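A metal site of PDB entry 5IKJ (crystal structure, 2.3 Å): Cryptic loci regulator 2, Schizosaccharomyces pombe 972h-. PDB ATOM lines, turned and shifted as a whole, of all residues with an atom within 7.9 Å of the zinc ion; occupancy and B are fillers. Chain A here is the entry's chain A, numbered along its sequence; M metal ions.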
ATOM      1  N   ASP A  21      -4.355 -33.415  19.977  1.00  0.00           N
ATOM      2  CA  ASP A  21      -5.663 -33.067  20.512  1.00  0.00           C
ATOM      3  C   ASP A  21      -6.161 -31.722  19.994  1.00  0.00           C
ATOM      4  O   ASP A  21      -7.194 -31.234  20.451  1.00  0.00           O
ATOM      5  CB  ASP A  21      -5.605 -33.034  22.037  1.00  0.00           C
ATOM      6  CG  ASP A  21      -4.761 -31.892  22.580  1.00  0.00           C
ATOM      7  OD1 ASP A  21      -3.855 -31.431  21.847  1.00  0.00           O
ATOM      8  OD2 ASP A  21      -5.000 -31.452  23.715  1.00  0.00           O
ATOM      9  N   TYR A 151      -3.223 -26.918  15.347  1.00  0.00           N
ATOM     10  CA  TYR A 151      -2.676 -25.796  16.108  1.00  0.00           C
ATOM     11  C   TYR A 151      -2.263 -24.685  15.147  1.00  0.00           C
ATOM     12  O   TYR A 151      -1.708 -24.951  14.076  1.00  0.00           O
ATOM     13  CB  TYR A 151      -1.481 -26.230  16.960  1.00  0.00           C
ATOM     14  CG  TYR A 151      -1.869 -26.888  18.264  1.00  0.00           C
ATOM     15  CD1 TYR A 151      -2.207 -28.237  18.314  1.00  0.00           C
ATOM     16  CD2 TYR A 151      -1.905 -26.174  19.455  1.00  0.00           C
ATOM     17  CE1 TYR A 151      -2.569 -28.843  19.506  1.00  0.00           C
ATOM     18  CE2 TYR A 151      -2.255 -26.769  20.642  1.00  0.00           C
ATOM     19  CZ  TYR A 151      -2.586 -28.112  20.664  1.00  0.00           C
ATOM     20  OH  TYR A 151      -2.950 -28.709  21.851  1.00  0.00           O
ATOM     21  N   HIS A 174      -5.671 -25.674  21.694  1.00  0.00           N
ATOM     22  CA  HIS A 174      -5.923 -26.455  22.888  1.00  0.00           C
ATOM     23  C   HIS A 174      -7.431 -26.599  23.109  1.00  0.00           C
ATOM     24  O   HIS A 174      -8.178 -25.628  22.914  1.00  0.00           O
ATOM     25  CB  HIS A 174      -5.272 -25.804  24.106  1.00  0.00           C
ATOM     26  CG  HIS A 174      -5.254 -26.679  25.323  1.00  0.00           C
ATOM     27  ND1 HIS A 174      -6.265 -26.692  26.245  1.00  0.00           N
ATOM     28  CD2 HIS A 174      -4.327 -27.565  25.769  1.00  0.00           C
ATOM     29  CE1 HIS A 174      -5.978 -27.550  27.208  1.00  0.00           C
ATOM     30  NE2 HIS A 174      -4.807 -28.092  26.941  1.00  0.00           N
ATOM     31  N   PRO A 175      -7.917 -27.785  23.508  1.00  0.00           N
ATOM     32  CA  PRO A 175      -9.372 -27.973  23.629  1.00  0.00           C
ATOM     33  C   PRO A 175     -10.064 -26.959  24.521  1.00  0.00           C
ATOM     34  O   PRO A 175     -11.262 -26.686  24.324  1.00  0.00           O
ATOM     35  CB  PRO A 175      -9.480 -29.393  24.206  1.00  0.00           C
ATOM     36  CG  PRO A 175      -8.248 -30.077  23.775  1.00  0.00           C
ATOM     37  CD  PRO A 175      -7.168 -29.027  23.760  1.00  0.00           C
ATOM     38  N   PHE A 180      -1.762 -20.809  24.159  1.00  0.00           N
ATOM     39  CA  PHE A 180      -0.466 -20.813  24.827  1.00  0.00           C
ATOM     40  C   PHE A 180       0.232 -19.515  24.451  1.00  0.00           C
ATOM     41  O   PHE A 180       0.602 -19.319  23.285  1.00  0.00           O
ATOM     42  CB  PHE A 180       0.375 -22.022  24.429  1.00  0.00           C
ATOM     43  CG  PHE A 180      -0.127 -23.328  24.982  1.00  0.00           C
ATOM     44  CD1 PHE A 180       0.168 -23.709  26.289  1.00  0.00           C
ATOM     45  CD2 PHE A 180      -0.867 -24.187  24.189  1.00  0.00           C
ATOM     46  CE1 PHE A 180      -0.274 -24.920  26.791  1.00  0.00           C
ATOM     47  CE2 PHE A 180      -1.324 -25.400  24.691  1.00  0.00           C
ATOM     48  CZ  PHE A 180      -1.025 -25.760  25.993  1.00  0.00           C
ATOM     49  N   ASP A 185       5.174 -22.236  27.560  1.00  0.00           N
ATOM     50  CA  ASP A 185       3.958 -22.842  28.104  1.00  0.00           C
ATOM     51  C   ASP A 185       3.466 -23.978  27.216  1.00  0.00           C
ATOM     52  O   ASP A 185       3.006 -25.013  27.718  1.00  0.00           O
ATOM     53  CB  ASP A 185       2.874 -21.785  28.267  1.00  0.00           C
ATOM     54  CG  ASP A 185       3.166 -20.809  29.395  1.00  0.00           C
ATOM     55  OD1 ASP A 185       4.009 -21.134  30.265  1.00  0.00           O
ATOM     56  OD2 ASP A 185       2.554 -19.725  29.413  1.00  0.00           O
ATOM     57  N   PHE A 186       3.552 -23.808  25.892  1.00  0.00           N
ATOM     58  CA  PHE A 186       3.159 -24.875  24.981  1.00  0.00           C
ATOM     59  C   PHE A 186       4.031 -26.114  25.138  1.00  0.00           C
ATOM     60  O   PHE A 186       3.544 -27.228  24.969  1.00  0.00           O
ATOM     61  CB  PHE A 186       3.210 -24.385  23.533  1.00  0.00           C
ATOM     62  CG  PHE A 186       3.117 -25.488  22.522  1.00  0.00           C
ATOM     63  CD1 PHE A 186       1.953 -26.217  22.382  1.00  0.00           C
ATOM     64  CD2 PHE A 186       4.199 -25.793  21.701  1.00  0.00           C
ATOM     65  CE1 PHE A 186       1.861 -27.235  21.451  1.00  0.00           C
ATOM     66  CE2 PHE A 186       4.107 -26.811  20.771  1.00  0.00           C
ATOM     67  CZ  PHE A 186       2.941 -27.533  20.643  1.00  0.00           C
ATOM     68  N   LEU A 187       5.303 -25.930  25.464  1.00  0.00           N
ATOM     69  CA  LEU A 187       6.242 -27.056  25.467  1.00  0.00           C
ATOM     70  C   LEU A 187       5.766 -28.169  26.381  1.00  0.00           C
ATOM     71  O   LEU A 187       5.909 -29.355  26.046  1.00  0.00           O
ATOM     72  CB  LEU A 187       7.635 -26.583  25.873  1.00  0.00           C
ATOM     73  CG  LEU A 187       8.647 -26.343  24.763  1.00  0.00           C
ATOM     74  CD1 LEU A 187       9.959 -25.889  25.362  1.00  0.00           C
ATOM     75  CD2 LEU A 187       8.859 -27.603  23.915  1.00  0.00           C
ATOM     76  N   HIS A 188       5.213 -27.833  27.543  1.00  0.00           N
ATOM     77  CA  HIS A 188       4.770 -28.868  28.463  1.00  0.00           C
ATOM     78  C   HIS A 188       3.623 -29.678  27.866  1.00  0.00           C
ATOM     79  O   HIS A 188       3.586 -30.904  28.035  1.00  0.00           O
ATOM     80  CB  HIS A 188       4.355 -28.233  29.792  1.00  0.00           C
ATOM     81  CG  HIS A 188       5.499 -27.641  30.553  1.00  0.00           C
ATOM     82  ND1 HIS A 188       6.365 -28.410  31.313  1.00  0.00           N
ATOM     83  CD2 HIS A 188       5.936 -26.366  30.668  1.00  0.00           C
ATOM     84  CE1 HIS A 188       7.273 -27.623  31.863  1.00  0.00           C
ATOM     85  NE2 HIS A 188       7.037 -26.386  31.481  1.00  0.00           N
ATOM     86  N   HIS A 189       2.699 -29.019  27.168  1.00  0.00           N
ATOM     87  CA  HIS A 189       1.645 -29.752  26.468  1.00  0.00           C
ATOM     88  C   HIS A 189       2.221 -30.547  25.305  1.00  0.00           C
ATOM     89  O   HIS A 189       1.826 -31.692  25.067  1.00  0.00           O
ATOM     90  CB  HIS A 189       0.565 -28.795  25.994  1.00  0.00           C
ATOM     91  CG  HIS A 189      -0.705 -29.478  25.589  1.00  0.00           C
ATOM     92  ND1 HIS A 189      -1.605 -29.970  26.500  1.00  0.00           N
ATOM     93  CD2 HIS A 189      -1.217 -29.748  24.363  1.00  0.00           C
ATOM     94  CE1 HIS A 189      -2.623 -30.516  25.866  1.00  0.00           C
ATOM     95  NE2 HIS A 189      -2.417 -30.397  24.569  1.00  0.00           N
ATOM     96  N   LEU A 190       3.149 -29.941  24.553  1.00  0.00           N
ATOM     97  CA  LEU A 190       3.813 -30.671  23.477  1.00  0.00           C
ATOM     98  C   LEU A 190       4.472 -31.943  24.003  1.00  0.00           C
ATOM     99  O   LEU A 190       4.356 -33.013  23.393  1.00  0.00           O
ATOM    100  CB  LEU A 190       4.864 -29.783  22.809  1.00  0.00           C
ATOM    101  CG  LEU A 190       5.676 -30.439  21.688  1.00  0.00           C
ATOM    102  CD1 LEU A 190       4.776 -30.857  20.532  1.00  0.00           C
ATOM    103  CD2 LEU A 190       6.781 -29.518  21.197  1.00  0.00           C
ATOM    104  N   TYR A 191       5.169 -31.847  25.140  1.00  0.00           N
ATOM    105  CA  TYR A 191       5.845 -33.000  25.703  1.00  0.00           C
ATOM    106  C   TYR A 191       4.848 -34.068  26.146  1.00  0.00           C
ATOM    107  O   TYR A 191       5.121 -35.262  26.039  1.00  0.00           O
ATOM    108  CB  TYR A 191       6.719 -32.550  26.878  1.00  0.00           C
ATOM    109  CG  TYR A 191       7.414 -33.669  27.606  1.00  0.00           C
ATOM    110  CD1 TYR A 191       8.574 -34.234  27.095  1.00  0.00           C
ATOM    111  CD2 TYR A 191       6.926 -34.149  28.815  1.00  0.00           C
ATOM    112  CE1 TYR A 191       9.221 -35.253  27.764  1.00  0.00           C
ATOM    113  CE2 TYR A 191       7.565 -35.166  29.491  1.00  0.00           C
ATOM    114  CZ  TYR A 191       8.717 -35.719  28.962  1.00  0.00           C
ATOM    115  OH  TYR A 191       9.349 -36.731  29.627  1.00  0.00           O
ATOM    116  N   TRP A 192       3.674 -33.648  26.637  1.00  0.00           N
ATOM    117  CA  TRP A 192       2.634 -34.602  27.005  1.00  0.00           C
ATOM    118  C   TRP A 192       2.084 -35.307  25.774  1.00  0.00           C
ATOM    119  O   TRP A 192       1.745 -36.496  25.834  1.00  0.00           O
ATOM    120  CB  TRP A 192       1.517 -33.889  27.765  1.00  0.00           C
ATOM    121  CG  TRP A 192       0.309 -34.735  28.015  1.00  0.00           C
ATOM    122  CD1 TRP A 192       0.160 -35.650  29.012  1.00  0.00           C
ATOM    123  CD2 TRP A 192      -0.906 -34.736  27.268  1.00  0.00           C
ATOM    124  NE1 TRP A 192      -1.092 -36.226  28.927  1.00  0.00           N
ATOM    125  CE2 TRP A 192      -1.760 -35.681  27.861  1.00  0.00           C
ATOM    126  CE3 TRP A 192      -1.360 -34.029  26.154  1.00  0.00           C
ATOM    127  CZ2 TRP A 192      -3.044 -35.948  27.384  1.00  0.00           C
ATOM    128  CZ3 TRP A 192      -2.631 -34.286  25.672  1.00  0.00           C
ATOM    129  CH2 TRP A 192      -3.457 -35.237  26.288  1.00  0.00           C
ATOM    130  N   LEU A 193       1.974 -34.600  24.649  1.00  0.00           N
ATOM    131  CA  LEU A 193       1.407 -35.194  23.447  1.00  0.00           C
ATOM    132  C   LEU A 193       2.264 -36.340  22.938  1.00  0.00           C
ATOM    133  O   LEU A 193       1.735 -37.344  22.440  1.00  0.00           O
ATOM    134  CB  LEU A 193       1.251 -34.127  22.356  1.00  0.00           C
ATOM    135  CG  LEU A 193       0.032 -33.210  22.456  1.00  0.00           C
ATOM    136  CD1 LEU A 193       0.126 -32.103  21.418  1.00  0.00           C
ATOM    137  CD2 LEU A 193      -1.258 -34.001  22.280  1.00  0.00           C
ATOM    138  N   ASN A 200      -3.989 -39.444  28.579  1.00  0.00           N
ATOM    139  CA  ASN A 200      -4.746 -39.036  29.765  1.00  0.00           C
ATOM    140  C   ASN A 200      -4.433 -37.580  30.063  1.00  0.00           C
ATOM    141  O   ASN A 200      -3.285 -37.220  30.335  1.00  0.00           O
ATOM    142  CB  ASN A 200      -4.404 -39.924  30.952  1.00  0.00           C
ATOM    143  CG  ASN A 200      -5.197 -39.575  32.204  1.00  0.00           C
ATOM    144  OD1 ASN A 200      -6.027 -38.661  32.183  1.00  0.00           O
ATOM    145  ND2 ASN A 200      -4.960 -40.307  33.283  1.00  0.00           N
ATOM    146  N   GLU A 201      -5.467 -36.735  30.028  1.00  0.00           N
ATOM    147  CA  GLU A 201      -5.284 -35.293  30.195  1.00  0.00           C
ATOM    148  C   GLU A 201      -4.792 -34.921  31.589  1.00  0.00           C
ATOM    149  O   GLU A 201      -4.322 -33.794  31.781  1.00  0.00           O
ATOM    150  CB  GLU A 201      -6.593 -34.570  29.886  1.00  0.00           C
ATOM    151  CG  GLU A 201      -7.153 -34.871  28.507  1.00  0.00           C
ATOM    152  CD  GLU A 201      -8.602 -35.338  28.541  1.00  0.00           C
ATOM    153  OE1 GLU A 201      -9.359 -34.869  29.407  1.00  0.00           O
ATOM    154  OE2 GLU A 201      -8.963 -36.193  27.697  1.00  0.00           O
ATOM    155  N   THR A 203      -2.253 -36.130  33.267  1.00  0.00           N
ATOM    156  CA  THR A 203      -0.822 -36.283  33.459  1.00  0.00           C
ATOM    157  C   THR A 203      -0.006 -35.160  32.837  1.00  0.00           C
ATOM    158  O   THR A 203       1.228 -35.207  32.875  1.00  0.00           O
ATOM    159  CB  THR A 203      -0.350 -37.621  32.872  1.00  0.00           C
ATOM    160  OG1 THR A 203      -0.279 -37.530  31.445  1.00  0.00           O
ATOM    161  CG2 THR A 203      -1.309 -38.746  33.255  1.00  0.00           C
ATOM    162  N   CYS A 204      -0.663 -34.145  32.276  1.00  0.00           N
ATOM    163  CA  CYS A 204       0.038 -33.022  31.657  1.00  0.00           C
ATOM    164  C   CYS A 204       0.304 -31.936  32.683  1.00  0.00           C
ATOM    165  O   CYS A 204      -0.541 -31.643  33.530  1.00  0.00           O
ATOM    166  CB  CYS A 204      -0.782 -32.448  30.498  1.00  0.00           C
ATOM    167  SG  CYS A 204       0.071 -31.170  29.545  1.00  0.00           S
ATOM    168  N   CYS A 205       1.494 -31.346  32.611  1.00  0.00           N
ATOM    169  CA  CYS A 205       1.901 -30.278  33.522  1.00  0.00           C
ATOM    170  C   CYS A 205       1.626 -28.882  32.965  1.00  0.00           C
ATOM    171  O   CYS A 205       1.895 -27.904  33.665  1.00  0.00           O
ATOM    172  CB  CYS A 205       3.388 -30.402  33.844  1.00  0.00           C
ATOM    173  SG  CYS A 205       3.915 -32.017  34.456  1.00  0.00           S
ATOM    174  N   CYS A 206       1.101 -28.767  31.753  1.00  0.00           N
ATOM    175  CA  CYS A 206       0.971 -27.469  31.123  1.00  0.00           C
ATOM    176  C   CYS A 206      -0.098 -26.634  31.822  1.00  0.00           C
ATOM    177  O   CYS A 206      -0.946 -27.149  32.553  1.00  0.00           O
ATOM    178  CB  CYS A 206       0.633 -27.607  29.638  1.00  0.00           C
ATOM    179  SG  CYS A 206      -1.127 -27.560  29.247  1.00  0.00           S
ATOM    180  N   VAL A 207      -0.049 -25.322  31.578  1.00  0.00           N
ATOM    181  CA  VAL A 207      -0.895 -24.395  32.322  1.00  0.00           C
ATOM    182  C   VAL A 207      -2.364 -24.599  31.985  1.00  0.00           C
ATOM    183  O   VAL A 207      -3.233 -24.389  32.838  1.00  0.00           O
ATOM    184  CB  VAL A 207      -0.466 -22.936  32.050  1.00  0.00           C
ATOM    185  CG1 VAL A 207      -1.122 -21.999  33.058  1.00  0.00           C
ATOM    186  CG2 VAL A 207       1.048 -22.791  32.095  1.00  0.00           C
ATOM    187  N   LEU A 208      -2.664 -24.999  30.755  1.00  0.00           N
ATOM    188  CA  LEU A 208      -4.057 -25.065  30.318  1.00  0.00           C
ATOM    189  C   LEU A 208      -4.745 -26.350  30.771  1.00  0.00           C
ATOM    190  O   LEU A 208      -5.974 -26.379  30.912  1.00  0.00           O
ATOM    191  CB  LEU A 208      -4.140 -24.929  28.803  1.00  0.00           C
ATOM    192  CG  LEU A 208      -3.626 -23.604  28.223  1.00  0.00           C
ATOM    193  CD1 LEU A 208      -3.785 -23.582  26.711  1.00  0.00           C
ATOM    194  CD2 LEU A 208      -4.315 -22.403  28.843  1.00  0.00           C
ATOM    195  N   CYS A 209      -3.985 -27.421  31.011  1.00  0.00           N
ATOM    196  CA  CYS A 209      -4.549 -28.640  31.563  1.00  0.00           C
ATOM    197  C   CYS A 209      -4.509 -28.675  33.078  1.00  0.00           C
ATOM    198  O   CYS A 209      -5.356 -29.327  33.701  1.00  0.00           O
ATOM    199  CB  CYS A 209      -3.794 -29.865  31.023  1.00  0.00           C
ATOM    200  SG  CYS A 209      -3.706 -29.968  29.225  1.00  0.00           S
ATOM    201  N   SER A 210      -3.554 -27.980  33.697  1.00  0.00           N
ATOM    202  CA  SER A 210      -3.334 -28.067  35.131  1.00  0.00           C
ATOM    203  C   SER A 210      -3.707 -26.805  35.900  1.00  0.00           C
ATOM    204  O   SER A 210      -3.910 -26.881  37.112  1.00  0.00           O
ATOM    205  CB  SER A 210      -1.861 -28.381  35.417  1.00  0.00           C
ATOM    206  OG  SER A 210      -1.507 -29.663  34.924  1.00  0.00           O
ATOM    207  N   ARG A 217       3.025 -29.820  39.587  1.00  0.00           N
ATOM    208  CA  ARG A 217       3.243 -30.907  38.635  1.00  0.00           C
ATOM    209  C   ARG A 217       4.586 -30.770  37.941  1.00  0.00           C
ATOM    210  O   ARG A 217       5.323 -31.750  37.799  1.00  0.00           O
ATOM    211  CB  ARG A 217       2.105 -30.941  37.609  1.00  0.00           C
ATOM    212  CG  ARG A 217       0.813 -31.552  38.122  1.00  0.00           C
ATOM    213  CD  ARG A 217      -0.275 -31.473  37.059  1.00  0.00           C
ATOM    214  NE  ARG A 217      -1.439 -32.296  37.358  1.00  0.00           N
ATOM    215  CZ  ARG A 217      -2.461 -32.475  36.534  1.00  0.00           C
ATOM    216  NH1 ARG A 217      -2.468 -31.881  35.340  1.00  0.00           N
ATOM    217  NH2 ARG A 217      -3.477 -33.238  36.881  1.00  0.00           N
HETATM  218 ZN    ZN M   1      -1.435 -29.832  28.590  1.00  0.00          ZN
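O of Cys 204 lies within hydrogen-bond range of OG of Ser 210.
A ring nitrogen (NE2) of His 189 sits at hydrogen-bond distance from the side-chain carboxylate (OD2) of Asp 21 (2.9 Å).
O of Cys 204 sits at hydrogen-bond distance from NH1 of Arg 217 (2.7 Å).
The side-chain sulfur of Cys 206 lies close to the backbone NH of Leu 208, at 3.3 Å.
NE2 of His 174 sits close to SG of Cys 209, at 3.2 Å.
The side-chain hydroxyl (OH) of Tyr 151 lies close to a ring nitrogen (NE2) of His 189, at 3.2 Å.
The zinc ion is bound by ND1 of His 189, SG of Cys 204, SG of Cys 209 and SG of Cys 206.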
